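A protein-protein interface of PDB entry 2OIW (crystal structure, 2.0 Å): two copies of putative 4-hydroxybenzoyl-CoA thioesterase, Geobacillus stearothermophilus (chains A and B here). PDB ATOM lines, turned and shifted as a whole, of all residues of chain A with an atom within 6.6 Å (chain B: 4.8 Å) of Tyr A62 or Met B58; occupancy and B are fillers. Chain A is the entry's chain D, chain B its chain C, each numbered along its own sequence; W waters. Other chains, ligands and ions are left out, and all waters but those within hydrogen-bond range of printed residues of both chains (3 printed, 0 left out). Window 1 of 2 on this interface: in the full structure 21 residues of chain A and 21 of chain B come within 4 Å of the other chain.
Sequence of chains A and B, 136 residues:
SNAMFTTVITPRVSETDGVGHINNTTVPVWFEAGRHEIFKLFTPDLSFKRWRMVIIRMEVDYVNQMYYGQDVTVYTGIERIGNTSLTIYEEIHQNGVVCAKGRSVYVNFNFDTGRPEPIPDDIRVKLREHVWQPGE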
ATOM      1  N   ASN A  23     -14.897 -22.575  -3.597  1.00  0.00           N
ATOM      2  CA  ASN A  23     -15.847 -21.478  -3.262  1.00  0.00           C
ATOM      3  C   ASN A  23     -16.268 -21.678  -1.801  1.00  0.00           C
ATOM      4  O   ASN A  23     -16.335 -22.820  -1.346  1.00  0.00           O
ATOM      5  CB  ASN A  23     -17.052 -21.516  -4.191  1.00  0.00           C
ATOM      6  CG  ASN A  23     -18.156 -20.556  -3.789  1.00  0.00           C
ATOM      7  OD1 ASN A  23     -19.121 -20.946  -3.114  1.00  0.00           O
ATOM      8  ND2 ASN A  23     -18.044 -19.320  -4.224  1.00  0.00           N
ATOM      9  N   ASN A  24     -16.543 -20.586  -1.070  1.00  0.00           N
ATOM     10  CA  ASN A  24     -16.894 -20.696   0.348  1.00  0.00           C
ATOM     11  C   ASN A  24     -18.077 -21.619   0.651  1.00  0.00           C
ATOM     12  O   ASN A  24     -18.120 -22.248   1.718  1.00  0.00           O
ATOM     13  CB  ASN A  24     -17.158 -19.326   0.965  1.00  0.00           C
ATOM     14  CG  ASN A  24     -18.371 -18.653   0.385  1.00  0.00           C
ATOM     15  OD1 ASN A  24     -19.472 -18.789   0.901  1.00  0.00           O
ATOM     16  ND2 ASN A  24     -18.188 -17.949  -0.696  1.00  0.00           N
ATOM     17  N   THR A  25     -19.042 -21.704  -0.257  1.00  0.00           N
ATOM     18  CA  THR A  25     -20.238 -22.534  -0.006  1.00  0.00           C
ATOM     19  C   THR A  25     -19.954 -24.050  -0.089  1.00  0.00           C
ATOM     20  O   THR A  25     -20.800 -24.879   0.300  1.00  0.00           O
ATOM     21  CB  THR A  25     -21.424 -22.160  -0.964  1.00  0.00           C
ATOM     22  OG1 THR A  25     -21.092 -22.493  -2.318  1.00  0.00           O
ATOM     23  CG2 THR A  25     -21.738 -20.667  -0.887  1.00  0.00           C
ATOM     24  N   THR A  26     -18.788 -24.404  -0.619  1.00  0.00           N
ATOM     25  CA  THR A  26     -18.341 -25.791  -0.668  1.00  0.00           C
ATOM     26  C   THR A  26     -17.953 -26.308   0.703  1.00  0.00           C
ATOM     27  O   THR A  26     -18.088 -27.507   1.012  1.00  0.00           O
ATOM     28  CB  THR A  26     -17.141 -25.915  -1.590  1.00  0.00           C
ATOM     29  OG1 THR A  26     -17.550 -25.557  -2.904  1.00  0.00           O
ATOM     30  CG2 THR A  26     -16.592 -27.352  -1.627  1.00  0.00           C
ATOM     31  N   VAL A  27     -17.470 -25.392   1.532  1.00  0.00           N
ATOM     32  CA  VAL A  27     -16.939 -25.783   2.806  1.00  0.00           C
ATOM     33  C   VAL A  27     -17.980 -26.479   3.734  1.00  0.00           C
ATOM     34  O   VAL A  27     -17.682 -27.510   4.330  1.00  0.00           O
ATOM     35  CB  VAL A  27     -16.180 -24.615   3.465  1.00  0.00           C
ATOM     36  CG1 VAL A  27     -15.933 -24.934   4.920  1.00  0.00           C
ATOM     37  CG2 VAL A  27     -14.852 -24.404   2.719  1.00  0.00           C
ATOM     38  N   PRO A  28     -19.171 -25.905   3.868  1.00  0.00           N
ATOM     39  CA  PRO A  28     -20.261 -26.578   4.596  1.00  0.00           C
ATOM     40  C   PRO A  28     -20.732 -27.898   3.977  1.00  0.00           C
ATOM     41  O   PRO A  28     -21.249 -28.768   4.679  1.00  0.00           O
ATOM     42  CB  PRO A  28     -21.396 -25.574   4.485  1.00  0.00           C
ATOM     43  CG  PRO A  28     -20.693 -24.203   4.368  1.00  0.00           C
ATOM     44  CD  PRO A  28     -19.556 -24.543   3.434  1.00  0.00           C
ATOM     45  N   MET A  58     -24.281 -22.957  12.751  1.00  0.00           N
ATOM     46  CA  MET A  58     -23.026 -23.260  12.079  1.00  0.00           C
ATOM     47  C   MET A  58     -22.074 -22.068  12.189  1.00  0.00           C
ATOM     48  O   MET A  58     -22.506 -20.917  12.045  1.00  0.00           O
ATOM     49  CB  MET A  58     -23.330 -23.583  10.617  1.00  0.00           C
ATOM     50  CG  MET A  58     -22.168 -23.877   9.762  1.00  0.00           C
ATOM     51  SD  MET A  58     -22.704 -23.726   7.871  1.00  0.00           S
ATOM     52  CE  MET A  58     -24.024 -25.198   7.839  1.00  0.00           C
ATOM     53  N   GLU A  59     -20.799 -22.349  12.465  1.00  0.00           N
ATOM     54  CA  GLU A  59     -19.736 -21.348  12.420  1.00  0.00           C
ATOM     55  C   GLU A  59     -18.598 -21.879  11.569  1.00  0.00           C
ATOM     56  O   GLU A  59     -18.187 -23.044  11.741  1.00  0.00           O
ATOM     57  CB  GLU A  59     -19.182 -21.071  13.818  1.00  0.00           C
ATOM     58  CG  GLU A  59     -20.247 -20.825  14.863  1.00  0.00           C
ATOM     59  CD  GLU A  59     -19.696 -20.646  16.301  1.00  0.00           C
ATOM     60  OE1 GLU A  59     -18.717 -21.317  16.704  1.00  0.00           O
ATOM     61  OE2 GLU A  59     -20.294 -19.845  17.047  1.00  0.00           O
ATOM     62  N   VAL A  60     -18.059 -21.047  10.678  1.00  0.00           N
ATOM     63  CA  VAL A  60     -16.879 -21.456   9.886  1.00  0.00           C
ATOM     64  C   VAL A  60     -15.791 -20.364   9.817  1.00  0.00           C
ATOM     65  O   VAL A  60     -16.076 -19.220   9.440  1.00  0.00           O
ATOM     66  CB  VAL A  60     -17.247 -21.851   8.439  1.00  0.00           C
ATOM     67  CG1 VAL A  60     -16.005 -22.319   7.704  1.00  0.00           C
ATOM     68  CG2 VAL A  60     -18.370 -22.909   8.388  1.00  0.00           C
ATOM     69  N   ASP A  61     -14.562 -20.719  10.201  1.00  0.00           N
ATOM     70  CA  ASP A  61     -13.410 -19.854   9.951  1.00  0.00           C
ATOM     71  C   ASP A  61     -12.663 -20.364   8.713  1.00  0.00           C
ATOM     72  O   ASP A  61     -12.231 -21.505   8.659  1.00  0.00           O
ATOM     73  CB  ASP A  61     -12.438 -19.808  11.130  1.00  0.00           C
ATOM     74  CG  ASP A  61     -13.018 -19.099  12.365  1.00  0.00           C
ATOM     75  OD1 ASP A  61     -13.620 -18.019  12.254  1.00  0.00           O
ATOM     76  OD2 ASP A  61     -12.836 -19.618  13.473  1.00  0.00           O
ATOM     77  N   TYR A  62     -12.558 -19.498   7.718  1.00  0.00           N
ATOM     78  CA  TYR A  62     -11.795 -19.755   6.523  1.00  0.00           C
ATOM     79  C   TYR A  62     -10.378 -19.219   6.700  1.00  0.00           C
ATOM     80  O   TYR A  62     -10.134 -17.997   6.566  1.00  0.00           O
ATOM     81  CB  TYR A  62     -12.477 -19.070   5.358  1.00  0.00           C
ATOM     82  CG  TYR A  62     -13.864 -19.599   5.062  1.00  0.00           C
ATOM     83  CD1 TYR A  62     -14.985 -19.062   5.698  1.00  0.00           C
ATOM     84  CD2 TYR A  62     -14.053 -20.608   4.120  1.00  0.00           C
ATOM     85  CE1 TYR A  62     -16.275 -19.533   5.410  1.00  0.00           C
ATOM     86  CE2 TYR A  62     -15.322 -21.071   3.826  1.00  0.00           C
ATOM     87  CZ  TYR A  62     -16.432 -20.526   4.461  1.00  0.00           C
ATOM     88  OH  TYR A  62     -17.687 -21.005   4.166  1.00  0.00           O
ATOM     89  N   VAL A  63      -9.468 -20.137   7.041  1.00  0.00           N
ATOM     90  CA  VAL A  63      -8.072 -19.840   7.428  1.00  0.00           C
ATOM     91  C   VAL A  63      -7.148 -19.702   6.207  1.00  0.00           C
ATOM     92  O   VAL A  63      -6.327 -18.785   6.133  1.00  0.00           O
ATOM     93  CB  VAL A  63      -7.526 -20.942   8.460  1.00  0.00           C
ATOM     94  CG1 VAL A  63      -6.157 -20.598   8.982  1.00  0.00           C
ATOM     95  CG2 VAL A  63      -8.489 -21.062   9.675  1.00  0.00           C
ATOM     96  N   ASN A  64      -7.260 -20.602   5.244  1.00  0.00           N
ATOM     97  CA  ASN A  64      -6.372 -20.564   4.083  1.00  0.00           C
ATOM     98  C   ASN A  64      -7.195 -21.019   2.895  1.00  0.00           C
ATOM     99  O   ASN A  64      -8.168 -21.786   3.070  1.00  0.00           O
ATOM    100  CB  ASN A  64      -5.200 -21.555   4.223  1.00  0.00           C
ATOM    101  CG  ASN A  64      -4.139 -21.132   5.255  1.00  0.00           C
ATOM    102  OD1 ASN A  64      -3.822 -21.903   6.166  1.00  0.00           O
ATOM    103  ND2 ASN A  64      -3.562 -19.962   5.090  1.00  0.00           N
ATOM    104  N   GLN A  65      -6.784 -20.576   1.700  1.00  0.00           N
ATOM    105  CA  GLN A  65      -7.412 -20.954   0.431  1.00  0.00           C
ATOM    106  C   GLN A  65      -7.206 -22.434   0.125  1.00  0.00           C
ATOM    107  O   GLN A  65      -6.149 -22.981   0.430  1.00  0.00           O
ATOM    108  CB  GLN A  65      -6.827 -20.109  -0.710  1.00  0.00           C
ATOM    109  CG  GLN A  65      -7.278 -18.617  -0.740  1.00  0.00           C
ATOM    110  CD  GLN A  65      -6.369 -17.628   0.002  1.00  0.00           C
ATOM    111  OE1 GLN A  65      -5.494 -17.998   0.802  1.00  0.00           O
ATOM    112  NE2 GLN A  65      -6.599 -16.340  -0.260  1.00  0.00           N
ATOM    113  N   MET A  66      -8.210 -23.078  -0.476  1.00  0.00           N
ATOM    114  CA  MET A  66      -8.056 -24.437  -0.953  1.00  0.00           C
ATOM    115  C   MET A  66      -8.235 -24.500  -2.449  1.00  0.00           C
ATOM    116  O   MET A  66      -8.907 -23.628  -3.073  1.00  0.00           O
ATOM    117  CB  MET A  66      -9.053 -25.345  -0.253  1.00  0.00           C
ATOM    118  CG  MET A  66      -8.655 -25.535   1.181  1.00  0.00           C
ATOM    119  SD  MET A  66      -9.741 -26.803   2.162  1.00  0.00           S
ATOM    120  CE  MET A  66     -11.209 -25.604   2.495  1.00  0.00           C
ATOM    121  N   CYS A  99      -7.140 -25.599   6.785  1.00  0.00           N
ATOM    122  CA  CYS A  99      -7.678 -24.533   5.925  1.00  0.00           C
ATOM    123  C   CYS A  99      -8.991 -23.928   6.351  1.00  0.00           C
ATOM    124  O   CYS A  99      -9.318 -22.819   5.956  1.00  0.00           O
ATOM    125  CB  CYS A  99      -7.747 -25.013   4.474  1.00  0.00           C
ATOM    126  SG  CYS A  99      -6.085 -25.234   3.769  1.00  0.00           S
ATOM    127  N   ALA A 100      -9.755 -24.664   7.133  1.00  0.00           N
ATOM    128  CA  ALA A 100     -11.071 -24.254   7.598  1.00  0.00           C
ATOM    129  C   ALA A 100     -11.320 -24.947   8.938  1.00  0.00           C
ATOM    130  O   ALA A 100     -10.882 -26.071   9.146  1.00  0.00           O
ATOM    131  CB  ALA A 100     -12.119 -24.643   6.594  1.00  0.00           C
ATOM    132  N   LYS A 101     -11.981 -24.248   9.853  1.00  0.00           N
ATOM    133  CA  LYS A 101     -12.269 -24.765  11.198  1.00  0.00           C
ATOM    134  C   LYS A 101     -13.699 -24.389  11.452  1.00  0.00           C
ATOM    135  O   LYS A 101     -14.099 -23.232  11.204  1.00  0.00           O
ATOM    136  CB  LYS A 101     -11.423 -24.068  12.257  1.00  0.00           C
ATOM    137  CG  LYS A 101      -9.966 -24.350  12.177  1.00  0.00           C
ATOM    138  CD  LYS A 101      -9.248 -23.594  13.284  1.00  0.00           C
ATOM    139  CE  LYS A 101      -7.722 -23.665  13.135  1.00  0.00           C
ATOM    140  NZ  LYS A 101      -7.001 -23.770  14.454  1.00  0.00           N
ATOM    141  N   PRO B  28     -26.051 -20.790   2.937  1.00  0.00           N
ATOM    142  CA  PRO B  28     -24.884 -19.997   2.489  1.00  0.00           C
ATOM    143  C   PRO B  28     -24.863 -19.653   0.999  1.00  0.00           C
ATOM    144  O   PRO B  28     -24.303 -18.623   0.622  1.00  0.00           O
ATOM    145  CB  PRO B  28     -23.692 -20.902   2.823  1.00  0.00           C
ATOM    146  CG  PRO B  28     -24.226 -21.816   3.946  1.00  0.00           C
ATOM    147  CD  PRO B  28     -25.639 -22.062   3.587  1.00  0.00           C
ATOM    148  N   ILE B  55     -13.831 -14.341   1.805  1.00  0.00           N
ATOM    149  CA  ILE B  55     -14.501 -14.546   3.069  1.00  0.00           C
ATOM    150  C   ILE B  55     -13.494 -15.077   4.101  1.00  0.00           C
ATOM    151  O   ILE B  55     -12.584 -15.846   3.756  1.00  0.00           O
ATOM    152  CB  ILE B  55     -15.785 -15.449   2.908  1.00  0.00           C
ATOM    153  CG1 ILE B  55     -16.689 -15.372   4.159  1.00  0.00           C
ATOM    154  CG2 ILE B  55     -15.399 -16.864   2.483  1.00  0.00           C
ATOM    155  CD1 ILE B  55     -18.110 -15.914   3.972  1.00  0.00           C
ATOM    156  N   ILE B  56     -13.613 -14.623   5.355  1.00  0.00           N
ATOM    157  CA  ILE B  56     -12.731 -15.109   6.418  1.00  0.00           C
ATOM    158  C   ILE B  56     -13.527 -15.795   7.529  1.00  0.00           C
ATOM    159  O   ILE B  56     -13.023 -16.683   8.213  1.00  0.00           O
ATOM    160  CB  ILE B  56     -11.722 -14.027   6.953  1.00  0.00           C
ATOM    161  CG1 ILE B  56     -12.408 -12.806   7.627  1.00  0.00           C
ATOM    162  CG2 ILE B  56     -10.805 -13.524   5.810  1.00  0.00           C
ATOM    163  CD1 ILE B  56     -11.429 -11.989   8.603  1.00  0.00           C
ATOM    164  N   ARG B  57     -14.799 -15.414   7.662  1.00  0.00           N
ATOM    165  CA  ARG B  57     -15.670 -15.972   8.699  1.00  0.00           C
ATOM    166  C   ARG B  57     -17.131 -15.958   8.284  1.00  0.00           C
ATOM    167  O   ARG B  57     -17.591 -15.004   7.644  1.00  0.00           O
ATOM    168  CB  ARG B  57     -15.508 -15.216  10.023  1.00  0.00           C
ATOM    169  CG  ARG B  57     -16.392 -15.791  11.114  1.00  0.00           C
ATOM    170  CD  ARG B  57     -15.899 -15.647  12.536  1.00  0.00           C
ATOM    171  NE  ARG B  57     -16.895 -16.218  13.470  1.00  0.00           N
ATOM    172  CZ  ARG B  57     -16.854 -17.443  14.004  1.00  0.00           C
ATOM    173  NH1 ARG B  57     -17.813 -17.827  14.841  1.00  0.00           N
ATOM    174  NH2 ARG B  57     -15.858 -18.287  13.724  1.00  0.00           N
ATOM    175  N   MET B  58     -17.856 -17.014   8.655  1.00  0.00           N
ATOM    176  CA  MET B  58     -19.303 -17.076   8.426  1.00  0.00           C
ATOM    177  C   MET B  58     -19.995 -17.719   9.629  1.00  0.00           C
ATOM    178  O   MET B  58     -19.464 -18.668  10.240  1.00  0.00           O
ATOM    179  CB  MET B  58     -19.556 -17.859   7.147  1.00  0.00           C
ATOM    180  CG  MET B  58     -20.966 -18.180   6.810  1.00  0.00           C
ATOM    181  SD  MET B  58     -21.061 -19.832   5.662  1.00  0.00           S
ATOM    182  CE  MET B  58     -20.233 -19.088   4.016  1.00  0.00           C
ATOM    183  N   GLU B  59     -21.160 -17.187  10.002  1.00  0.00           N
ATOM    184  CA  GLU B  59     -22.030 -17.882  10.963  1.00  0.00           C
ATOM    185  C   GLU B  59     -23.484 -17.856  10.539  1.00  0.00           C
ATOM    186  O   GLU B  59     -23.963 -16.866   9.940  1.00  0.00           O
ATOM    187  CB  GLU B  59     -21.847 -17.380  12.412  1.00  0.00           C
ATOM    188  CG  GLU B  59     -22.033 -15.910  12.572  1.00  0.00           C
ATOM    189  CD  GLU B  59     -21.227 -15.339  13.734  1.00  0.00           C
ATOM    190  OE1 GLU B  59     -19.959 -15.343  13.672  1.00  0.00           O
ATOM    191  OE2 GLU B  59     -21.880 -14.898  14.712  1.00  0.00           O
ATOM    192  N   VAL B  60     -24.172 -18.966  10.787  1.00  0.00           N
ATOM    193  CA  VAL B  60     -25.565 -19.083  10.382  1.00  0.00           C
ATOM    194  C   VAL B  60     -26.346 -19.616  11.553  1.00  0.00           C
ATOM    195  O   VAL B  60     -25.954 -20.623  12.142  1.00  0.00           O
ATOM    196  CB  VAL B  60     -25.767 -20.019   9.155  1.00  0.00           C
ATOM    197  CG1 VAL B  60     -27.254 -20.013   8.676  1.00  0.00           C
ATOM    198  CG2 VAL B  60     -24.843 -19.582   8.015  1.00  0.00           C
ATOM    199  N   ARG B 103     -24.118 -13.854   9.733  1.00  0.00           N
ATOM    200  CA  ARG B 103     -23.137 -12.800   9.834  1.00  0.00           C
ATOM    201  C   ARG B 103     -21.929 -13.330   9.096  1.00  0.00           C
ATOM    202  O   ARG B 103     -21.503 -14.460   9.319  1.00  0.00           O
ATOM    203  CB  ARG B 103     -22.840 -12.547  11.316  1.00  0.00           C
ATOM    204  CG  ARG B 103     -22.268 -11.190  11.646  1.00  0.00           C
ATOM    205  CD  ARG B 103     -22.362 -10.865  13.156  1.00  0.00           C
ATOM    206  NE  ARG B 103     -23.436  -9.904  13.453  1.00  0.00           N
ATOM    207  CZ  ARG B 103     -24.554 -10.187  14.136  1.00  0.00           C
ATOM    208  NH1 ARG B 103     -24.773 -11.405  14.607  1.00  0.00           N
ATOM    209  NH2 ARG B 103     -25.469  -9.249  14.348  1.00  0.00           N
ATOM    210  N   SER B 104     -21.423 -12.569   8.147  1.00  0.00           N
ATOM    211  CA  SER B 104     -20.210 -12.987   7.453  1.00  0.00           C
ATOM    212  C   SER B 104     -19.174 -11.865   7.442  1.00  0.00           C
ATOM    213  O   SER B 104     -19.534 -10.676   7.437  1.00  0.00           O
ATOM    214  CB  SER B 104     -20.496 -13.499   6.048  1.00  0.00           C
ATOM    215  OG  SER B 104     -21.173 -12.522   5.290  1.00  0.00           O
HETATM  216  O   HOH W   1     -21.873 -17.688   1.927  1.00  0.00           O
HETATM  217  O   HOH W   2     -11.740 -16.367  10.609  1.00  0.00           O
HETATM  218  O   HOH W   3     -10.048 -16.636   4.104  1.00  0.00           O
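The side-chain amide oxygen (OD1) of Asn A23 is in hydrogen-bond range of the side-chain hydroxyl (OG1) of Thr A25.
The guanidinium group (NE) of Arg B57 lies within salt-bridge range of the side-chain carboxylate (OE1) of Glu B59 (3.2 Å).
The backbone carbonyl oxygen (O) of Asn A24 is in hydrogen-bond range of the side-chain hydroxyl (OH) of Tyr A62.
N of Glu B59 is in hydrogen-bond range of O of Arg B103 (2.8 Å).
N of Asp A61 lies within hydrogen-bond range of O of Lys A101 (2.7 Å).
Water W3 bridges O of Ile B55 and O of Tyr A62.
Water W2 lies within hydrogen-bond range of O of Ile B56 (2.7 Å) and OD1 of Asp A61 (3.0 Å).
Water W1 lies within hydrogen-bond range of the side-chain amide oxygen (OD1) of Asn A24 (2.8 Å) and the backbone carbonyl oxygen (O) of Pro B28 (2.9 Å).
Met A58 touches Glu B59, and with the chains exchanged Glu A59 touches Met B58.
Met A58 touches Val B60, and with the chains exchanged Val A60 touches Met B58.
Of the 14 pairs that touch across the chains among the printed residues, 4 have their exchanged pair printed and touching as well.
Asn A24 touches Ile B55.
OD1 of Asn A24 touches CE of Met B58 (3.2 Å).
Pro B28 touches Thr A25.
Glu B59 touches Met A58.
CA of Glu A59 touches O of Met B58, 3.5 Å away.
Val A60 touches Arg B57 (O to CA, 3.4 Å).
Asp A61 touches Ile B56 (CA to O, 3.6 Å).
Tyr A62 touches Ile B55 (CB to O, 3.6 Å).
Met B58 touches Tyr A62 (CE to OH, 3.2 Å).
Val A27 touches none of the printed residues of chain B.
Of the printed residues of chain B, Glu A59 touches Arg B57 (3.7 Å) and Met B58 (3.5 Å).
Tyr A62 touches three residues of chain B.
Ala A100 touches none of the printed residues of chain B.
Printed residues of chain A within 4 Å of Ile B55: Asn A24 (3.4 Å) and Tyr A62 (3.6 Å).
Met B58 touches just these residues of chain A: Asn A24 (3.2 Å), Glu A59 (3.5 Å), Val A60 (2.8 Å) and Tyr A62 (3.2 Å).
The nearest printed residue of chain B that does not touch Glu A59 is Glu B59 (4.4 Å).
N of Tyr A62 lies within hydrogen-bond range of O of Ile B56, 2.9 Å away.
The guanidinium group (NH2) of Arg B57 lies within salt-bridge range of the side-chain carboxylate (OD1) of Asp A61, 2.7 Å away.
The backbone NH (N) of Val B60 lies within hydrogen-bond range of the backbone carbonyl oxygen (O) of Met A58.
The backbone carbonyl oxygen of Met B58 is in hydrogen-bond range of the backbone NH of Val A60, 2.8 Å away.
NH1 of Arg B57 lies within salt-bridge range of OE2 of Glu A59, 3.9 Å away.
Of the 18 printed residues of chain A, 7 touch a printed residue of chain B.
Along chain A the printed residues that touch a printed residue of chain B span positions 24 to 62.
Among the printed residues, 14 pairs touch across the chains.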
